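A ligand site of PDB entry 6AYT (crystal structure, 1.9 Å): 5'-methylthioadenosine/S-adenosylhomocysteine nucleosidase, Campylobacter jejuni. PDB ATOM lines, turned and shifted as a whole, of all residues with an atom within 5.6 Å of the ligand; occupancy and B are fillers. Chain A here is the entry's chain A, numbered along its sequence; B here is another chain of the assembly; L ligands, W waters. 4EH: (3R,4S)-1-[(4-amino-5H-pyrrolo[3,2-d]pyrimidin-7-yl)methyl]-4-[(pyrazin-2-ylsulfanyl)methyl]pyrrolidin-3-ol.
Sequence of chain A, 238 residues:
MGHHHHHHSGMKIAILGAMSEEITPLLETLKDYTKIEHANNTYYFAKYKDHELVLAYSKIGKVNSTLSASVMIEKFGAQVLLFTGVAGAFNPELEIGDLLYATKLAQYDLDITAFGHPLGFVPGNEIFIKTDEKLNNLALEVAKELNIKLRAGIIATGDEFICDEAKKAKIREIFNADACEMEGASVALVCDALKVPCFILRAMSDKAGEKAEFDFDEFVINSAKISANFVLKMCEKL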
ATOM      1  N   ALA A  18     -11.509  -5.647  23.061  1.00  0.00           N
ATOM      2  CA  ALA A  18     -10.611  -6.811  23.146  1.00  0.00           C
ATOM      3  C   ALA A  18      -9.577  -6.847  22.007  1.00  0.00           C
ATOM      4  O   ALA A  18      -8.405  -7.151  22.237  1.00  0.00           O
ATOM      5  CB  ALA A  18     -11.420  -8.104  23.176  1.00  0.00           C
ATOM      6  N   MET A  19     -10.034  -6.542  20.792  1.00  0.00           N
ATOM      7  CA  MET A  19      -9.247  -6.686  19.559  1.00  0.00           C
ATOM      8  C   MET A  19      -8.999  -5.316  18.925  1.00  0.00           C
ATOM      9  O   MET A  19      -9.786  -4.397  19.093  1.00  0.00           O
ATOM     10  CB  MET A  19     -10.020  -7.551  18.548  1.00  0.00           C
ATOM     11  CG  MET A  19     -10.373  -8.920  19.074  1.00  0.00           C
ATOM     12  SD  MET A  19     -11.307  -9.972  17.999  1.00  0.00           S
ATOM     13  CE  MET A  19     -10.104 -10.305  16.707  1.00  0.00           C
ATOM     14  N   GLU A  22     -11.831  -3.518  17.169  1.00  0.00           N
ATOM     15  CA  GLU A  22     -12.869  -2.895  17.989  1.00  0.00           C
ATOM     16  C   GLU A  22     -12.532  -1.477  18.454  1.00  0.00           C
ATOM     17  O   GLU A  22     -13.420  -0.730  18.884  1.00  0.00           O
ATOM     18  CB  GLU A  22     -13.184  -3.811  19.179  1.00  0.00           C
ATOM     19  CG  GLU A  22     -13.741  -5.164  18.729  1.00  0.00           C
ATOM     20  CD  GLU A  22     -13.785  -6.224  19.817  1.00  0.00           C
ATOM     21  OE1 GLU A  22     -12.885  -6.263  20.684  1.00  0.00           O
ATOM     22  OE2 GLU A  22     -14.718  -7.048  19.813  1.00  0.00           O
ATOM     23  N   ILE A  60      -7.500 -10.769  23.862  1.00  0.00           N
ATOM     24  CA  ILE A  60      -8.718 -11.574  24.059  1.00  0.00           C
ATOM     25  C   ILE A  60      -8.763 -12.231  25.422  1.00  0.00           C
ATOM     26  O   ILE A  60      -7.744 -12.654  25.952  1.00  0.00           O
ATOM     27  CB  ILE A  60      -8.716 -12.740  23.001  1.00  0.00           C
ATOM     28  CG1 ILE A  60      -8.731 -12.242  21.572  1.00  0.00           C
ATOM     29  CG2 ILE A  60      -9.823 -13.742  23.234  1.00  0.00           C
ATOM     30  CD1 ILE A  60      -9.609 -11.073  21.340  1.00  0.00           C
ATOM     31  N   GLY A  61      -9.980 -12.314  25.990  1.00  0.00           N
ATOM     32  CA  GLY A  61     -10.230 -13.165  27.143  1.00  0.00           C
ATOM     33  C   GLY A  61     -10.362 -12.458  28.471  1.00  0.00           C
ATOM     34  O   GLY A  61     -10.150 -11.248  28.593  1.00  0.00           O
ATOM     35  N   VAL A  86     -17.592  -6.763  19.639  1.00  0.00           N
ATOM     36  CA  VAL A  86     -18.537  -7.652  18.966  1.00  0.00           C
ATOM     37  C   VAL A  86     -18.863  -8.856  19.836  1.00  0.00           C
ATOM     38  O   VAL A  86     -18.203  -9.089  20.871  1.00  0.00           O
ATOM     39  CB  VAL A  86     -18.032  -8.057  17.554  1.00  0.00           C
ATOM     40  CG1 VAL A  86     -17.771  -6.804  16.716  1.00  0.00           C
ATOM     41  CG2 VAL A  86     -16.801  -8.937  17.589  1.00  0.00           C
ATOM     42  N   ALA A  87     -19.894  -9.613  19.457  1.00  0.00           N
ATOM     43  CA  ALA A  87     -20.337 -10.769  20.242  1.00  0.00           C
ATOM     44  C   ALA A  87     -21.083 -11.797  19.387  1.00  0.00           C
ATOM     45  O   ALA A  87     -21.497 -11.496  18.260  1.00  0.00           O
ATOM     46  CB  ALA A  87     -21.220 -10.294  21.399  1.00  0.00           C
ATOM     47  N   GLY A  88     -21.235 -12.998  19.938  1.00  0.00           N
ATOM     48  CA  GLY A  88     -22.014 -14.060  19.310  1.00  0.00           C
ATOM     49  C   GLY A  88     -23.447 -14.023  19.822  1.00  0.00           C
ATOM     50  O   GLY A  88     -23.676 -14.094  21.027  1.00  0.00           O
ATOM     51  N   GLU A 160     -13.913 -19.316  25.959  1.00  0.00           N
ATOM     52  CA  GLU A 160     -14.055 -20.111  24.752  1.00  0.00           C
ATOM     53  C   GLU A 160     -14.782 -19.332  23.656  1.00  0.00           C
ATOM     54  O   GLU A 160     -15.746 -18.635  23.939  1.00  0.00           O
ATOM     55  CB  GLU A 160     -14.818 -21.391  25.078  1.00  0.00           C
ATOM     56  CG  GLU A 160     -14.816 -22.408  23.942  1.00  0.00           C
ATOM     57  CD  GLU A 160     -15.656 -23.635  24.227  1.00  0.00           C
ATOM     58  OE1 GLU A 160     -16.021 -23.881  25.394  1.00  0.00           O
ATOM     59  OE2 GLU A 160     -15.930 -24.360  23.236  1.00  0.00           O
ATOM     60  N   PHE A 161     -14.307 -19.442  22.409  1.00  0.00           N
ATOM     61  CA  PHE A 161     -15.090 -18.981  21.259  1.00  0.00           C
ATOM     62  C   PHE A 161     -16.180 -20.015  20.988  1.00  0.00           C
ATOM     63  O   PHE A 161     -15.885 -21.166  20.664  1.00  0.00           O
ATOM     64  CB  PHE A 161     -14.221 -18.796  19.995  1.00  0.00           C
ATOM     65  CG  PHE A 161     -14.985 -18.236  18.824  1.00  0.00           C
ATOM     66  CD1 PHE A 161     -15.194 -16.885  18.703  1.00  0.00           C
ATOM     67  CD2 PHE A 161     -15.472 -19.083  17.832  1.00  0.00           C
ATOM     68  CE1 PHE A 161     -15.893 -16.353  17.617  1.00  0.00           C
ATOM     69  CE2 PHE A 161     -16.188 -18.561  16.736  1.00  0.00           C
ATOM     70  CZ  PHE A 161     -16.388 -17.187  16.635  1.00  0.00           C
ATOM     71  N   ILE A 162     -17.444 -19.623  21.155  1.00  0.00           N
ATOM     72  CA  ILE A 162     -18.577 -20.537  21.038  1.00  0.00           C
ATOM     73  C   ILE A 162     -19.000 -20.666  19.570  1.00  0.00           C
ATOM     74  O   ILE A 162     -19.415 -19.686  18.941  1.00  0.00           O
ATOM     75  CB  ILE A 162     -19.781 -20.078  21.887  1.00  0.00           C
ATOM     76  CG1 ILE A 162     -19.393 -19.972  23.369  1.00  0.00           C
ATOM     77  CG2 ILE A 162     -20.957 -21.027  21.710  1.00  0.00           C
ATOM     78  CD1 ILE A 162     -18.831 -21.233  24.005  1.00  0.00           C
ATOM     79  N   CYS A 163     -18.894 -21.891  19.028  1.00  0.00           N
ATOM     80  CA  CYS A 163     -19.251 -22.170  17.637  1.00  0.00           C
ATOM     81  C   CYS A 163     -19.813 -23.595  17.544  1.00  0.00           C
ATOM     82  O   CYS A 163     -19.345 -24.419  16.770  1.00  0.00           O
ATOM     83  CB  CYS A 163     -18.033 -21.974  16.738  1.00  0.00           C
ATOM     84  SG  CYS A 163     -16.592 -22.928  17.260  1.00  0.00           S
ATOM     85  N   CYS A 180     -22.964 -14.134  23.773  1.00  0.00           N
ATOM     86  CA  CYS A 180     -21.739 -14.567  24.437  1.00  0.00           C
ATOM     87  C   CYS A 180     -20.536 -13.804  23.911  1.00  0.00           C
ATOM     88  O   CYS A 180     -20.533 -13.276  22.777  1.00  0.00           O
ATOM     89  CB  CYS A 180     -21.503 -16.064  24.289  1.00  0.00           C
ATOM     90  SG  CYS A 180     -21.108 -16.619  22.608  1.00  0.00           S
ATOM     91  N   GLU A 181     -19.524 -13.712  24.753  1.00  0.00           N
ATOM     92  CA  GLU A 181     -18.240 -13.095  24.414  1.00  0.00           C
ATOM     93  C   GLU A 181     -17.233 -13.502  25.503  1.00  0.00           C
ATOM     94  O   GLU A 181     -17.521 -14.377  26.319  1.00  0.00           O
ATOM     95  CB  GLU A 181     -18.398 -11.576  24.187  1.00  0.00           C
ATOM     96  CG  GLU A 181     -19.434 -10.846  25.048  1.00  0.00           C
ATOM     97  CD  GLU A 181     -18.878 -10.357  26.345  1.00  0.00           C
ATOM     98  OE1 GLU A 181     -19.035  -9.149  26.634  1.00  0.00           O
ATOM     99  OE2 GLU A 181     -18.250 -11.165  27.084  1.00  0.00           O
ATOM    100  N   MET A 182     -16.047 -12.895  25.508  1.00  0.00           N
ATOM    101  CA  MET A 182     -14.945 -13.383  26.317  1.00  0.00           C
ATOM    102  C   MET A 182     -14.346 -12.331  27.260  1.00  0.00           C
ATOM    103  O   MET A 182     -13.285 -12.575  27.838  1.00  0.00           O
ATOM    104  CB  MET A 182     -13.863 -13.961  25.367  1.00  0.00           C
ATOM    105  CG  MET A 182     -14.373 -15.061  24.438  1.00  0.00           C
ATOM    106  SD  MET A 182     -13.147 -15.676  23.238  1.00  0.00           S
ATOM    107  CE  MET A 182     -11.919 -16.377  24.290  1.00  0.00           C
ATOM    108  N   GLU A 183     -15.017 -11.194  27.430  1.00  0.00           N
ATOM    109  CA  GLU A 183     -14.482 -10.075  28.228  1.00  0.00           C
ATOM    110  C   GLU A 183     -15.483  -9.319  29.121  1.00  0.00           C
ATOM    111  O   GLU A 183     -15.048  -8.600  30.022  1.00  0.00           O
ATOM    112  CB  GLU A 183     -13.796  -9.059  27.316  1.00  0.00           C
ATOM    113  CG  GLU A 183     -12.663  -9.602  26.442  1.00  0.00           C
ATOM    114  CD  GLU A 183     -13.103 -10.316  25.178  1.00  0.00           C
ATOM    115  OE1 GLU A 183     -14.292 -10.207  24.764  1.00  0.00           O
ATOM    116  OE2 GLU A 183     -12.249 -11.017  24.581  1.00  0.00           O
ATOM    117  N   ARG A 202     -22.137  -4.506  22.805  1.00  0.00           N
ATOM    118  CA  ARG A 202     -21.690  -5.451  21.799  1.00  0.00           C
ATOM    119  C   ARG A 202     -22.569  -5.378  20.553  1.00  0.00           C
ATOM    120  O   ARG A 202     -23.793  -5.335  20.663  1.00  0.00           O
ATOM    121  CB  ARG A 202     -21.713  -6.866  22.370  1.00  0.00           C
ATOM    122  CG  ARG A 202     -20.832  -7.082  23.595  1.00  0.00           C
ATOM    123  CD  ARG A 202     -19.345  -7.038  23.246  1.00  0.00           C
ATOM    124  NE  ARG A 202     -18.508  -7.634  24.289  1.00  0.00           N
ATOM    125  CZ  ARG A 202     -17.271  -8.126  24.128  1.00  0.00           C
ATOM    126  NH1 ARG A 202     -16.672  -8.136  22.936  1.00  0.00           N
ATOM    127  NH2 ARG A 202     -16.616  -8.614  25.177  1.00  0.00           N
ATOM    128  N   SER A 205     -21.550 -10.196  15.674  1.00  0.00           N
ATOM    129  CA  SER A 205     -20.717 -10.595  14.527  1.00  0.00           C
ATOM    130  C   SER A 205     -21.040 -11.976  13.962  1.00  0.00           C
ATOM    131  O   SER A 205     -20.605 -12.318  12.863  1.00  0.00           O
ATOM    132  CB  SER A 205     -19.245 -10.583  14.931  1.00  0.00           C
ATOM    133  OG  SER A 205     -19.038 -11.422  16.053  1.00  0.00           O
ATOM    134  N   ASP A 206     -21.767 -12.775  14.729  1.00  0.00           N
ATOM    135  CA  ASP A 206     -22.098 -14.160  14.352  1.00  0.00           C
ATOM    136  C   ASP A 206     -23.212 -14.669  15.276  1.00  0.00           C
ATOM    137  O   ASP A 206     -23.662 -13.935  16.169  1.00  0.00           O
ATOM    138  CB  ASP A 206     -20.858 -15.064  14.455  1.00  0.00           C
ATOM    139  CG  ASP A 206     -20.250 -15.060  15.838  1.00  0.00           C
ATOM    140  OD1 ASP A 206     -19.405 -14.176  16.134  1.00  0.00           O
ATOM    141  OD2 ASP A 206     -20.623 -15.930  16.646  1.00  0.00           O
ATOM    142  N   ALA A 208     -22.918 -17.799  16.866  1.00  0.00           N
ATOM    143  CA  ALA A 208     -22.304 -18.743  17.813  1.00  0.00           C
ATOM    144  C   ALA A 208     -22.602 -20.230  17.560  1.00  0.00           C
ATOM    145  O   ALA A 208     -22.495 -21.041  18.479  1.00  0.00           O
ATOM    146  CB  ALA A 208     -22.708 -18.355  19.239  1.00  0.00           C
ATOM    147  N   ALA A 212     -19.769 -20.164  12.857  1.00  0.00           N
ATOM    148  CA  ALA A 212     -19.609 -18.875  13.563  1.00  0.00           C
ATOM    149  C   ALA A 212     -18.242 -18.225  13.315  1.00  0.00           C
ATOM    150  O   ALA A 212     -18.165 -17.007  13.214  1.00  0.00           O
ATOM    151  CB  ALA A 212     -19.850 -19.058  15.059  1.00  0.00           C
ATOM    152  N   PHE A 216     -17.872 -14.566  11.797  1.00  0.00           N
ATOM    153  CA  PHE A 216     -17.025 -13.620  12.532  1.00  0.00           C
ATOM    154  C   PHE A 216     -16.023 -12.916  11.605  1.00  0.00           C
ATOM    155  O   PHE A 216     -15.939 -11.694  11.598  1.00  0.00           O
ATOM    156  CB  PHE A 216     -16.279 -14.319  13.672  1.00  0.00           C
ATOM    157  CG  PHE A 216     -15.351 -13.422  14.406  1.00  0.00           C
ATOM    158  CD1 PHE A 216     -15.797 -12.661  15.485  1.00  0.00           C
ATOM    159  CD2 PHE A 216     -14.021 -13.289  13.992  1.00  0.00           C
ATOM    160  CE1 PHE A 216     -14.937 -11.802  16.144  1.00  0.00           C
ATOM    161  CE2 PHE A 216     -13.164 -12.416  14.652  1.00  0.00           C
ATOM    162  CZ  PHE A 216     -13.621 -11.687  15.732  1.00  0.00           C
ATOM    163  N   ILE B 112      -9.438 -20.375  21.557  1.00  0.00           N
ATOM    164  CA  ILE B 112      -9.872 -19.901  20.243  1.00  0.00           C
ATOM    165  C   ILE B 112      -9.312 -20.835  19.171  1.00  0.00           C
ATOM    166  O   ILE B 112      -8.916 -20.398  18.072  1.00  0.00           O
ATOM    167  CB  ILE B 112      -9.520 -18.418  19.993  1.00  0.00           C
ATOM    168  CG1 ILE B 112      -8.013 -18.140  20.151  1.00  0.00           C
ATOM    169  CG2 ILE B 112     -10.326 -17.511  20.928  1.00  0.00           C
ATOM    170  CD1 ILE B 112      -7.622 -16.771  19.632  1.00  0.00           C
ATOM    171  N   PHE B 115     -10.161 -20.916  15.303  1.00  0.00           N
ATOM    172  CA  PHE B 115      -9.375 -20.130  14.349  1.00  0.00           C
ATOM    173  C   PHE B 115      -7.974 -20.685  14.078  1.00  0.00           C
ATOM    174  O   PHE B 115      -7.133 -19.983  13.510  1.00  0.00           O
ATOM    175  CB  PHE B 115      -9.292 -18.670  14.840  1.00  0.00           C
ATOM    176  CG  PHE B 115     -10.625 -18.002  14.880  1.00  0.00           C
ATOM    177  CD1 PHE B 115     -11.437 -18.089  16.019  1.00  0.00           C
ATOM    178  CD2 PHE B 115     -11.107 -17.325  13.765  1.00  0.00           C
ATOM    179  CE1 PHE B 115     -12.691 -17.498  16.041  1.00  0.00           C
ATOM    180  CE2 PHE B 115     -12.363 -16.721  13.788  1.00  0.00           C
ATOM    181  CZ  PHE B 115     -13.147 -16.802  14.931  1.00  0.00           C
ATOM    182  N   HIS B 117      -5.542 -21.668  16.235  1.00  0.00           N
ATOM    183  CA  HIS B 117      -4.514 -21.446  17.240  1.00  0.00           C
ATOM    184  C   HIS B 117      -4.406 -22.639  18.169  1.00  0.00           C
ATOM    185  O   HIS B 117      -5.379 -23.387  18.326  1.00  0.00           O
ATOM    186  CB  HIS B 117      -4.817 -20.202  18.059  1.00  0.00           C
ATOM    187  CG  HIS B 117      -4.950 -18.948  17.252  1.00  0.00           C
ATOM    188  ND1 HIS B 117      -3.864 -18.340  16.644  1.00  0.00           N
ATOM    189  CD2 HIS B 117      -6.018 -18.207  16.916  1.00  0.00           C
ATOM    190  CE1 HIS B 117      -4.277 -17.265  15.997  1.00  0.00           C
ATOM    191  NE2 HIS B 117      -5.579 -17.167  16.144  1.00  0.00           N
ATOM    192  N   PRO B 123      -3.508 -14.157  20.417  1.00  0.00           N
ATOM    193  CA  PRO B 123      -2.572 -13.202  19.800  1.00  0.00           C
ATOM    194  C   PRO B 123      -2.066 -12.135  20.778  1.00  0.00           C
ATOM    195  O   PRO B 123      -2.832 -11.617  21.605  1.00  0.00           O
ATOM    196  CB  PRO B 123      -3.414 -12.554  18.705  1.00  0.00           C
ATOM    197  CG  PRO B 123      -4.393 -13.603  18.318  1.00  0.00           C
ATOM    198  CD  PRO B 123      -4.715 -14.338  19.588  1.00  0.00           C
HETATM  199  O3' 4EH L   1     -12.471 -11.060  21.941  1.00  0.00           O
HETATM  200  C3' 4EH L   1     -12.932 -12.381  21.622  1.00  0.00           C
HETATM  201  C4' 4EH L   1     -12.855 -12.721  20.143  1.00  0.00           C
HETATM  202  C5' 4EH L   1     -12.689 -14.229  19.948  1.00  0.00           C
HETATM  203  S   4EH L   1     -12.484 -14.647  18.250  1.00  0.00           S
HETATM  204  C2' 4EH L   1     -14.417 -12.412  21.884  1.00  0.00           C
HETATM  205  N1' 4EH L   1     -14.903 -11.661  20.723  1.00  0.00           N
HETATM  206  C1' 4EH L   1     -14.142 -12.167  19.546  1.00  0.00           C
HETATM  207  C10 4EH L   1     -16.359 -11.580  20.645  1.00  0.00           C
HETATM  208  C9  4EH L   1     -17.095 -12.743  20.045  1.00  0.00           C
HETATM  209  C4  4EH L   1     -17.271 -14.118  20.512  1.00  0.00           C
HETATM  210  N3  4EH L   1     -16.786 -14.722  21.628  1.00  0.00           N
HETATM  211  C2  4EH L   1     -17.084 -16.005  21.835  1.00  0.00           C
HETATM  212  C8  4EH L   1     -17.816 -12.694  18.862  1.00  0.00           C
HETATM  213  N7  4EH L   1     -18.391 -13.904  18.616  1.00  0.00           N
HETATM  214  C5  4EH L   1     -18.061 -14.782  19.579  1.00  0.00           C
HETATM  215  C6  4EH L   1     -18.341 -16.115  19.843  1.00  0.00           C
HETATM  216  N1  4EH L   1     -17.846 -16.703  20.967  1.00  0.00           N
HETATM  217  N6  4EH L   1     -19.121 -16.831  18.986  1.00  0.00           N
HETATM  218  C6' 4EH L   1     -10.910 -14.316  17.706  1.00  0.00           C
HETATM  219  C9' 4EH L   1     -10.540 -14.608  16.391  1.00  0.00           C
HETATM  220  N3' 4EH L   1      -9.294 -14.340  15.957  1.00  0.00           N
HETATM  221  C8' 4EH L   1      -8.399 -13.794  16.788  1.00  0.00           C
HETATM  222  C7' 4EH L   1      -8.770 -13.501  18.103  1.00  0.00           C
HETATM  223  N2' 4EH L   1     -10.011 -13.762  18.541  1.00  0.00           N
HETATM  224  O   HOH W   1     -17.699 -16.971  25.133  1.00  0.00           O
HETATM  225  O   HOH W   2     -14.415  -9.081  21.441  1.00  0.00           O
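The backbone NH (N) of Gly 88 sits close to a nitrogen (N7) of the ligand, at 3.3 Å. The side-chain carboxylate (OD1) of Asp 206 lies within hydrogen-bond range of a nitrogen (N7) of the ligand (2.7 Å). The side-chain carboxylate (OE2) of Glu 183 sits at hydrogen-bond distance from an oxygen (O3') of the ligand, at 2.6 Å. The side-chain sulfur (SG) of Cys 180 is in hydrogen-bond range of a nitrogen (N1) of the ligand. The backbone NH of Ile 162 sits at hydrogen-bond distance from a nitrogen (N1) of the ligand (3.0 Å). The backbone carbonyl oxygen (O) of Ile 162 sits at hydrogen-bond distance from a nitrogen (N6) of the ligand.
OD2 of Asp 206 is in hydrogen-bond range of N of Ala 208 (3.0 Å). OE2 of Glu 183 lies within hydrogen-bond range of N of Gly 61 (3.0 Å). The backbone carbonyl oxygen (O) of Ala 87 lies within hydrogen-bond range of the backbone NH (N) of Ser 205, at 2.9 Å. NH2 of Arg 202 lies within salt-bridge range of OE1 of Glu 183, 2.8 Å away. The side-chain carboxylate (OD1) of Asp 206 lies within hydrogen-bond range of the side-chain hydroxyl (OG) of Ser 205, at 2.8 Å. O of Gly 88 sits at hydrogen-bond distance from N of Cys 180, at 2.8 Å. The guanidinium group (NE) of Arg 202 is in salt-bridge range of the side-chain carboxylate (OE1) of Glu 181, 2.8 Å away. The backbone NH of Glu 183 lies within hydrogen-bond range of the side-chain carboxylate of Glu 181 (3.3 Å).
CB of Ala 18 touches O3' of the ligand, 3.4 Å away. CE of Met 19 touches C7' of the ligand (3.7 Å). CD1 of Ile 60 touches O3' of the ligand (2.9 Å). Val 86 touches the ligand (O to C10, 3.1 Å). Ala 87 touches the ligand (C to C8, 3.4 Å). O of Glu 160 touches C2 of the ligand, at 3.6 Å. Phe 161 touches the ligand. Glu 181 touches the ligand. Met 182 touches the ligand. OG of Ser 205 touches C8 of the ligand (3.3 Å). Ala 208 touches the ligand (CA to N6, 3.9 Å). Phe 216 touches the ligand (CE1 to C1', 3.5 Å). Ile 112 of chain B touches the ligand. CE1 of Phe 115 of chain B touches S of the ligand, at 3.6 Å.
Water W2 lies within hydrogen-bond range of OE2 of Glu 22 (2.6 Å), O3' of the ligand (2.8 Å) and NH1 of Arg 202 (2.9 Å). Water W1 lies within hydrogen-bond range of O of Glu 160 (2.8 Å) and O of Glu 181 (2.9 Å).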
